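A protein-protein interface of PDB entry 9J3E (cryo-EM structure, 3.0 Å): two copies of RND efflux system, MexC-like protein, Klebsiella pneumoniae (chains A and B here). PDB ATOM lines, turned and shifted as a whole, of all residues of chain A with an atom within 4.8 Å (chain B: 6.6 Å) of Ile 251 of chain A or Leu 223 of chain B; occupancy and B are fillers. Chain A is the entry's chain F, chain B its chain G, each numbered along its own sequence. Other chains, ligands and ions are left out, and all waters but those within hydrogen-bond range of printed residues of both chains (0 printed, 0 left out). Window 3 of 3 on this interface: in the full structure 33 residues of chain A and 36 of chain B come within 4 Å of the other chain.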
ATOM      1  N   LEU A 244       2.760  -1.281 -17.670  1.00  0.00           N
ATOM      2  CA  LEU A 244       1.635  -2.157 -17.952  1.00  0.00           C
ATOM      3  C   LEU A 244       0.353  -1.356 -17.822  1.00  0.00           C
ATOM      4  O   LEU A 244       0.168  -0.637 -16.837  1.00  0.00           O
ATOM      5  CB  LEU A 244       1.621  -3.340 -16.985  1.00  0.00           C
ATOM      6  CG  LEU A 244       0.734  -4.545 -17.267  1.00  0.00           C
ATOM      7  CD1 LEU A 244      -0.643  -4.350 -16.674  1.00  0.00           C
ATOM      8  CD2 LEU A 244       0.649  -4.761 -18.750  1.00  0.00           C
ATOM      9  N   ARG A 245      -0.521  -1.469 -18.811  1.00  0.00           N
ATOM     10  CA  ARG A 245      -1.816  -0.810 -18.763  1.00  0.00           C
ATOM     11  C   ARG A 245      -2.904  -1.817 -19.083  1.00  0.00           C
ATOM     12  O   ARG A 245      -2.943  -2.359 -20.191  1.00  0.00           O
ATOM     13  CB  ARG A 245      -1.887   0.354 -19.742  1.00  0.00           C
ATOM     14  CG  ARG A 245      -3.117   1.201 -19.548  1.00  0.00           C
ATOM     15  CD  ARG A 245      -3.069   2.426 -20.419  1.00  0.00           C
ATOM     16  NE  ARG A 245      -3.115   2.058 -21.826  1.00  0.00           N
ATOM     17  CZ  ARG A 245      -4.217   2.076 -22.562  1.00  0.00           C
ATOM     18  NH1 ARG A 245      -5.386   2.411 -22.044  1.00  0.00           N
ATOM     19  NH2 ARG A 245      -4.144   1.742 -23.847  1.00  0.00           N
ATOM     20  N   VAL A 246      -3.792  -2.049 -18.129  1.00  0.00           N
ATOM     21  CA  VAL A 246      -4.869  -3.010 -18.316  1.00  0.00           C
ATOM     22  C   VAL A 246      -5.906  -2.407 -19.248  1.00  0.00           C
ATOM     23  O   VAL A 246      -6.330  -1.260 -19.068  1.00  0.00           O
ATOM     24  CB  VAL A 246      -5.484  -3.406 -16.969  1.00  0.00           C
ATOM     25  CG1 VAL A 246      -6.803  -4.115 -17.180  1.00  0.00           C
ATOM     26  CG2 VAL A 246      -4.522  -4.287 -16.204  1.00  0.00           C
ATOM     27  N   THR A 249      -9.243  -0.089 -18.468  1.00  0.00           N
ATOM     28  CA  THR A 249      -9.132   0.492 -17.141  1.00  0.00           C
ATOM     29  C   THR A 249      -7.938   1.433 -17.096  1.00  0.00           C
ATOM     30  O   THR A 249      -7.081   1.434 -17.982  1.00  0.00           O
ATOM     31  CB  THR A 249      -8.978  -0.584 -16.058  1.00  0.00           C
ATOM     32  OG1 THR A 249      -7.615  -1.021 -16.018  1.00  0.00           O
ATOM     33  CG2 THR A 249      -9.874  -1.775 -16.337  1.00  0.00           C
ATOM     34  N   ASP A 250      -7.889   2.239 -16.040  1.00  0.00           N
ATOM     35  CA  ASP A 250      -6.765   3.124 -15.778  1.00  0.00           C
ATOM     36  C   ASP A 250      -5.700   2.455 -14.928  1.00  0.00           C
ATOM     37  O   ASP A 250      -4.738   3.111 -14.519  1.00  0.00           O
ATOM     38  CB  ASP A 250      -7.247   4.404 -15.100  1.00  0.00           C
ATOM     39  CG  ASP A 250      -8.597   4.859 -15.610  1.00  0.00           C
ATOM     40  OD1 ASP A 250      -9.451   5.238 -14.782  1.00  0.00           O
ATOM     41  OD2 ASP A 250      -8.805   4.836 -16.840  1.00  0.00           O
ATOM     42  N   ILE A 251      -5.857   1.164 -14.652  1.00  0.00           N
ATOM     43  CA  ILE A 251      -4.914   0.444 -13.810  1.00  0.00           C
ATOM     44  C   ILE A 251      -3.573   0.356 -14.524  1.00  0.00           C
ATOM     45  O   ILE A 251      -3.436  -0.340 -15.535  1.00  0.00           O
ATOM     46  CB  ILE A 251      -5.455  -0.946 -13.462  1.00  0.00           C
ATOM     47  CG1 ILE A 251      -6.842  -0.817 -12.837  1.00  0.00           C
ATOM     48  CG2 ILE A 251      -4.513  -1.665 -12.536  1.00  0.00           C
ATOM     49  CD1 ILE A 251      -7.610  -2.105 -12.787  1.00  0.00           C
ATOM     50  N   GLU A 252      -2.579   1.062 -13.997  1.00  0.00           N
ATOM     51  CA  GLU A 252      -1.226   1.051 -14.528  1.00  0.00           C
ATOM     52  C   GLU A 252      -0.311   0.308 -13.570  1.00  0.00           C
ATOM     53  O   GLU A 252      -0.451   0.427 -12.351  1.00  0.00           O
ATOM     54  CB  GLU A 252      -0.688   2.461 -14.735  1.00  0.00           C
ATOM     55  CG  GLU A 252       0.579   2.501 -15.563  1.00  0.00           C
ATOM     56  CD  GLU A 252       1.067   3.909 -15.819  1.00  0.00           C
ATOM     57  OE1 GLU A 252       0.235   4.840 -15.809  1.00  0.00           O
ATOM     58  OE2 GLU A 252       2.285   4.087 -16.023  1.00  0.00           O
ATOM     59  N   ARG A 253       0.614  -0.468 -14.125  1.00  0.00           N
ATOM     60  CA  ARG A 253       1.594  -1.198 -13.339  1.00  0.00           C
ATOM     61  C   ARG A 253       2.937  -1.127 -14.044  1.00  0.00           C
ATOM     62  O   ARG A 253       2.996  -1.075 -15.274  1.00  0.00           O
ATOM     63  CB  ARG A 253       1.171  -2.654 -13.149  1.00  0.00           C
ATOM     64  CG  ARG A 253      -0.060  -2.786 -12.292  1.00  0.00           C
ATOM     65  CD  ARG A 253       0.185  -2.271 -10.897  1.00  0.00           C
ATOM     66  NE  ARG A 253      -0.983  -2.481 -10.058  1.00  0.00           N
ATOM     67  CZ  ARG A 253      -2.017  -1.653 -10.038  1.00  0.00           C
ATOM     68  NH1 ARG A 253      -2.042  -0.567 -10.793  1.00  0.00           N
ATOM     69  NH2 ARG A 253      -3.044  -1.915  -9.239  1.00  0.00           N
ATOM     70  N   VAL A 283      -4.751  -7.314  -8.552  1.00  0.00           N
ATOM     71  CA  VAL A 283      -5.567  -6.775  -9.635  1.00  0.00           C
ATOM     72  C   VAL A 283      -5.224  -7.443 -10.960  1.00  0.00           C
ATOM     73  O   VAL A 283      -6.116  -7.825 -11.725  1.00  0.00           O
ATOM     74  CB  VAL A 283      -5.395  -5.251  -9.711  1.00  0.00           C
ATOM     75  CG1 VAL A 283      -3.939  -4.892  -9.527  1.00  0.00           C
ATOM     76  CG2 VAL A 283      -5.896  -4.739 -11.037  1.00  0.00           C
ATOM     77  N   LEU A 285      -4.916  -9.951 -13.342  1.00  0.00           N
ATOM     78  CA  LEU A 285      -5.442 -11.302 -13.375  1.00  0.00           C
ATOM     79  C   LEU A 285      -4.796 -12.109 -14.491  1.00  0.00           C
ATOM     80  O   LEU A 285      -4.529 -11.582 -15.572  1.00  0.00           O
ATOM     81  CB  LEU A 285      -6.958 -11.281 -13.578  1.00  0.00           C
ATOM     82  CG  LEU A 285      -7.755 -10.524 -12.518  1.00  0.00           C
ATOM     83  CD1 LEU A 285      -9.231 -10.546 -12.842  1.00  0.00           C
ATOM     84  CD2 LEU A 285      -7.502 -11.122 -11.153  1.00  0.00           C
ATOM     85  N   MET A 288      -5.592 -12.252 -18.677  1.00  0.00           N
ATOM     86  CA  MET A 288      -6.177 -11.000 -19.128  1.00  0.00           C
ATOM     87  C   MET A 288      -5.319 -10.365 -20.206  1.00  0.00           C
ATOM     88  O   MET A 288      -4.090 -10.385 -20.126  1.00  0.00           O
ATOM     89  CB  MET A 288      -6.322 -10.040 -17.958  1.00  0.00           C
ATOM     90  CG  MET A 288      -6.903  -8.707 -18.337  1.00  0.00           C
ATOM     91  SD  MET A 288      -8.683  -8.732 -18.196  1.00  0.00           S
ATOM     92  CE  MET A 288      -8.789  -8.672 -16.420  1.00  0.00           C
ATOM     93  N   PRO B 218     -18.007  -9.970 -17.041  1.00  0.00           N
ATOM     94  CA  PRO B 218     -16.888  -9.359 -17.760  1.00  0.00           C
ATOM     95  C   PRO B 218     -15.805  -8.926 -16.789  1.00  0.00           C
ATOM     96  O   PRO B 218     -16.084  -8.344 -15.741  1.00  0.00           O
ATOM     97  CB  PRO B 218     -17.529  -8.159 -18.460  1.00  0.00           C
ATOM     98  CG  PRO B 218     -18.950  -8.537 -18.606  1.00  0.00           C
ATOM     99  CD  PRO B 218     -19.291  -9.345 -17.392  1.00  0.00           C
ATOM    100  N   ALA B 219     -14.558  -9.222 -17.143  1.00  0.00           N
ATOM    101  CA  ALA B 219     -13.472  -8.936 -16.219  1.00  0.00           C
ATOM    102  C   ALA B 219     -13.350  -7.448 -15.952  1.00  0.00           C
ATOM    103  O   ALA B 219     -13.377  -7.029 -14.791  1.00  0.00           O
ATOM    104  CB  ALA B 219     -12.162  -9.489 -16.760  1.00  0.00           C
ATOM    105  N   ALA B 220     -13.274  -6.636 -17.009  1.00  0.00           N
ATOM    106  CA  ALA B 220     -13.075  -5.203 -16.835  1.00  0.00           C
ATOM    107  C   ALA B 220     -14.118  -4.610 -15.898  1.00  0.00           C
ATOM    108  O   ALA B 220     -13.813  -3.708 -15.112  1.00  0.00           O
ATOM    109  CB  ALA B 220     -13.106  -4.503 -18.190  1.00  0.00           C
ATOM    110  N   ASP B 221     -15.350  -5.117 -15.953  1.00  0.00           N
ATOM    111  CA  ASP B 221     -16.354  -4.688 -14.990  1.00  0.00           C
ATOM    112  C   ASP B 221     -15.949  -5.061 -13.574  1.00  0.00           C
ATOM    113  O   ASP B 221     -16.148  -4.279 -12.638  1.00  0.00           O
ATOM    114  CB  ASP B 221     -17.710  -5.297 -15.331  1.00  0.00           C
ATOM    115  CG  ASP B 221     -18.209  -4.870 -16.689  1.00  0.00           C
ATOM    116  OD1 ASP B 221     -17.405  -4.322 -17.470  1.00  0.00           O
ATOM    117  OD2 ASP B 221     -19.406  -5.077 -16.975  1.00  0.00           O
ATOM    118  N   ALA B 222     -15.386  -6.254 -13.393  1.00  0.00           N
ATOM    119  CA  ALA B 222     -14.948  -6.654 -12.063  1.00  0.00           C
ATOM    120  C   ALA B 222     -13.841  -5.743 -11.550  1.00  0.00           C
ATOM    121  O   ALA B 222     -13.866  -5.327 -10.389  1.00  0.00           O
ATOM    122  CB  ALA B 222     -14.490  -8.111 -12.070  1.00  0.00           C
ATOM    123  N   LEU B 223     -12.866  -5.410 -12.398  1.00  0.00           N
ATOM    124  CA  LEU B 223     -11.817  -4.504 -11.941  1.00  0.00           C
ATOM    125  C   LEU B 223     -12.360  -3.110 -11.670  1.00  0.00           C
ATOM    126  O   LEU B 223     -11.903  -2.436 -10.746  1.00  0.00           O
ATOM    127  CB  LEU B 223     -10.653  -4.420 -12.927  1.00  0.00           C
ATOM    128  CG  LEU B 223      -9.880  -5.657 -13.376  1.00  0.00           C
ATOM    129  CD1 LEU B 223      -9.662  -6.606 -12.212  1.00  0.00           C
ATOM    130  CD2 LEU B 223     -10.509  -6.339 -14.548  1.00  0.00           C
ATOM    131  N   ARG B 224     -13.317  -2.645 -12.473  1.00  0.00           N
ATOM    132  CA  ARG B 224     -13.871  -1.317 -12.230  1.00  0.00           C
ATOM    133  C   ARG B 224     -14.631  -1.271 -10.914  1.00  0.00           C
ATOM    134  O   ARG B 224     -14.493  -0.313 -10.143  1.00  0.00           O
ATOM    135  CB  ARG B 224     -14.769  -0.902 -13.388  1.00  0.00           C
ATOM    136  CG  ARG B 224     -13.999  -0.531 -14.625  1.00  0.00           C
ATOM    137  CD  ARG B 224     -14.923  -0.021 -15.691  1.00  0.00           C
ATOM    138  NE  ARG B 224     -14.550  -0.553 -16.993  1.00  0.00           N
ATOM    139  CZ  ARG B 224     -15.318  -1.357 -17.711  1.00  0.00           C
ATOM    140  NH1 ARG B 224     -16.509  -1.740 -17.282  1.00  0.00           N
ATOM    141  NH2 ARG B 224     -14.880  -1.792 -18.888  1.00  0.00           N
ATOM    142  N   LEU B 225     -15.434  -2.297 -10.634  1.00  0.00           N
ATOM    143  CA  LEU B 225     -16.125  -2.356  -9.351  1.00  0.00           C
ATOM    144  C   LEU B 225     -15.136  -2.464  -8.202  1.00  0.00           C
ATOM    145  O   LEU B 225     -15.316  -1.833  -7.155  1.00  0.00           O
ATOM    146  CB  LEU B 225     -17.094  -3.532  -9.326  1.00  0.00           C
ATOM    147  CG  LEU B 225     -17.566  -3.944  -7.933  1.00  0.00           C
ATOM    148  CD1 LEU B 225     -18.363  -2.832  -7.280  1.00  0.00           C
ATOM    149  CD2 LEU B 225     -18.375  -5.224  -7.998  1.00  0.00           C
ATOM    150  N   ARG B 226     -14.093  -3.281  -8.392  1.00  0.00           N
ATOM    151  CA  ARG B 226     -13.054  -3.455  -7.342  1.00  0.00           C
ATOM    152  C   ARG B 226     -12.405  -2.096  -7.073  1.00  0.00           C
ATOM    153  O   ARG B 226     -12.211  -1.761  -5.889  1.00  0.00           O
ATOM    154  CB  ARG B 226     -12.025  -4.505  -7.778  1.00  0.00           C
ATOM    155  CG  ARG B 226     -10.605  -4.238  -7.301  1.00  0.00           C
ATOM    156  CD  ARG B 226      -9.567  -5.037  -8.065  1.00  0.00           C
ATOM    157  NE  ARG B 226      -8.771  -5.866  -7.171  1.00  0.00           N
ATOM    158  CZ  ARG B 226      -8.530  -7.158  -7.357  1.00  0.00           C
ATOM    159  NH1 ARG B 226      -9.022  -7.777  -8.416  1.00  0.00           N
ATOM    160  NH2 ARG B 226      -7.797  -7.826  -6.484  1.00  0.00           N
ATOM    161  N   ALA B 227     -12.099  -1.340  -8.132  1.00  0.00           N
ATOM    162  CA  ALA B 227     -11.512  -0.019  -7.964  1.00  0.00           C
ATOM    163  C   ALA B 227     -12.463   0.905  -7.222  1.00  0.00           C
ATOM    164  O   ALA B 227     -12.064   1.580  -6.267  1.00  0.00           O
ATOM    165  CB  ALA B 227     -11.148   0.569  -9.325  1.00  0.00           C
ATOM    166  N   ALA B 228     -13.733   0.922  -7.622  1.00  0.00           N
ATOM    167  CA  ALA B 228     -14.695   1.789  -6.952  1.00  0.00           C
ATOM    168  C   ALA B 228     -14.797   1.449  -5.473  1.00  0.00           C
ATOM    169  O   ALA B 228     -14.916   2.345  -4.631  1.00  0.00           O
ATOM    170  CB  ALA B 228     -16.058   1.685  -7.628  1.00  0.00           C
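Of chain B, only Leu 223 comes within 4 Å of Ile 251 of chain A.
Of the printed residues of chain B, Val 283 of chain A touches Leu 223 (3.8 Å) and Arg 226 (3.7 Å).
Printed residues of chain B within 4 Å of Met 288 of chain A: Ala 219 (3.5 Å) and Leu 223 (3.5 Å).
Printed residues of chain A within 4 Å of Leu 223 of chain B: Ile 251, Val 283 and Met 288.
Printed residues of chain A within 4 Å of Arg 226 of chain B: Val 283 (3.7 Å).
The nearest residue of chain B that does not touch Ile 251 of chain A is Ala 227 of chain B (5.6 Å).
The backbone NH (N) of Val 246 of chain A sits at hydrogen-bond distance from the backbone carbonyl oxygen (O) of Ile 251 of chain A (3.1 Å).
The side-chain hydroxyl of Thr 249 of chain A sits at hydrogen-bond distance from the backbone NH of Ile 251 of chain A (3.1 Å).
CD1 of Ile 251 of chain A touches CB of Leu 223 of chain B (3.8 Å).
CD1 of Leu 223 of chain B touches O of Val 283 of chain A, 3.8 Å away.
Val 283 of chain A touches Arg 226 of chain B (N to NH2, 3.7 Å).
Met 288 of chain A touches Ala 219 of chain B.
Met 288 of chain A touches Leu 223 of chain B (CE to CD2, 3.5 Å).
Hydrophobic or aromatic side chains of chain A that line the printed part of chain B: Ile 251 and Met 288.
Printed residues of chain B that touch a printed residue of chain A: Ala 219, Leu 223 and Arg 226.
Hydrophobic or aromatic side chains of chain B within 4 Å of the printed part of chain A: Ala 219 and Leu 223.
No position is printed for both chains.
Of the 5 pairs that touch across the chains among the printed residues, none has its exchanged pair printed and touching as well.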
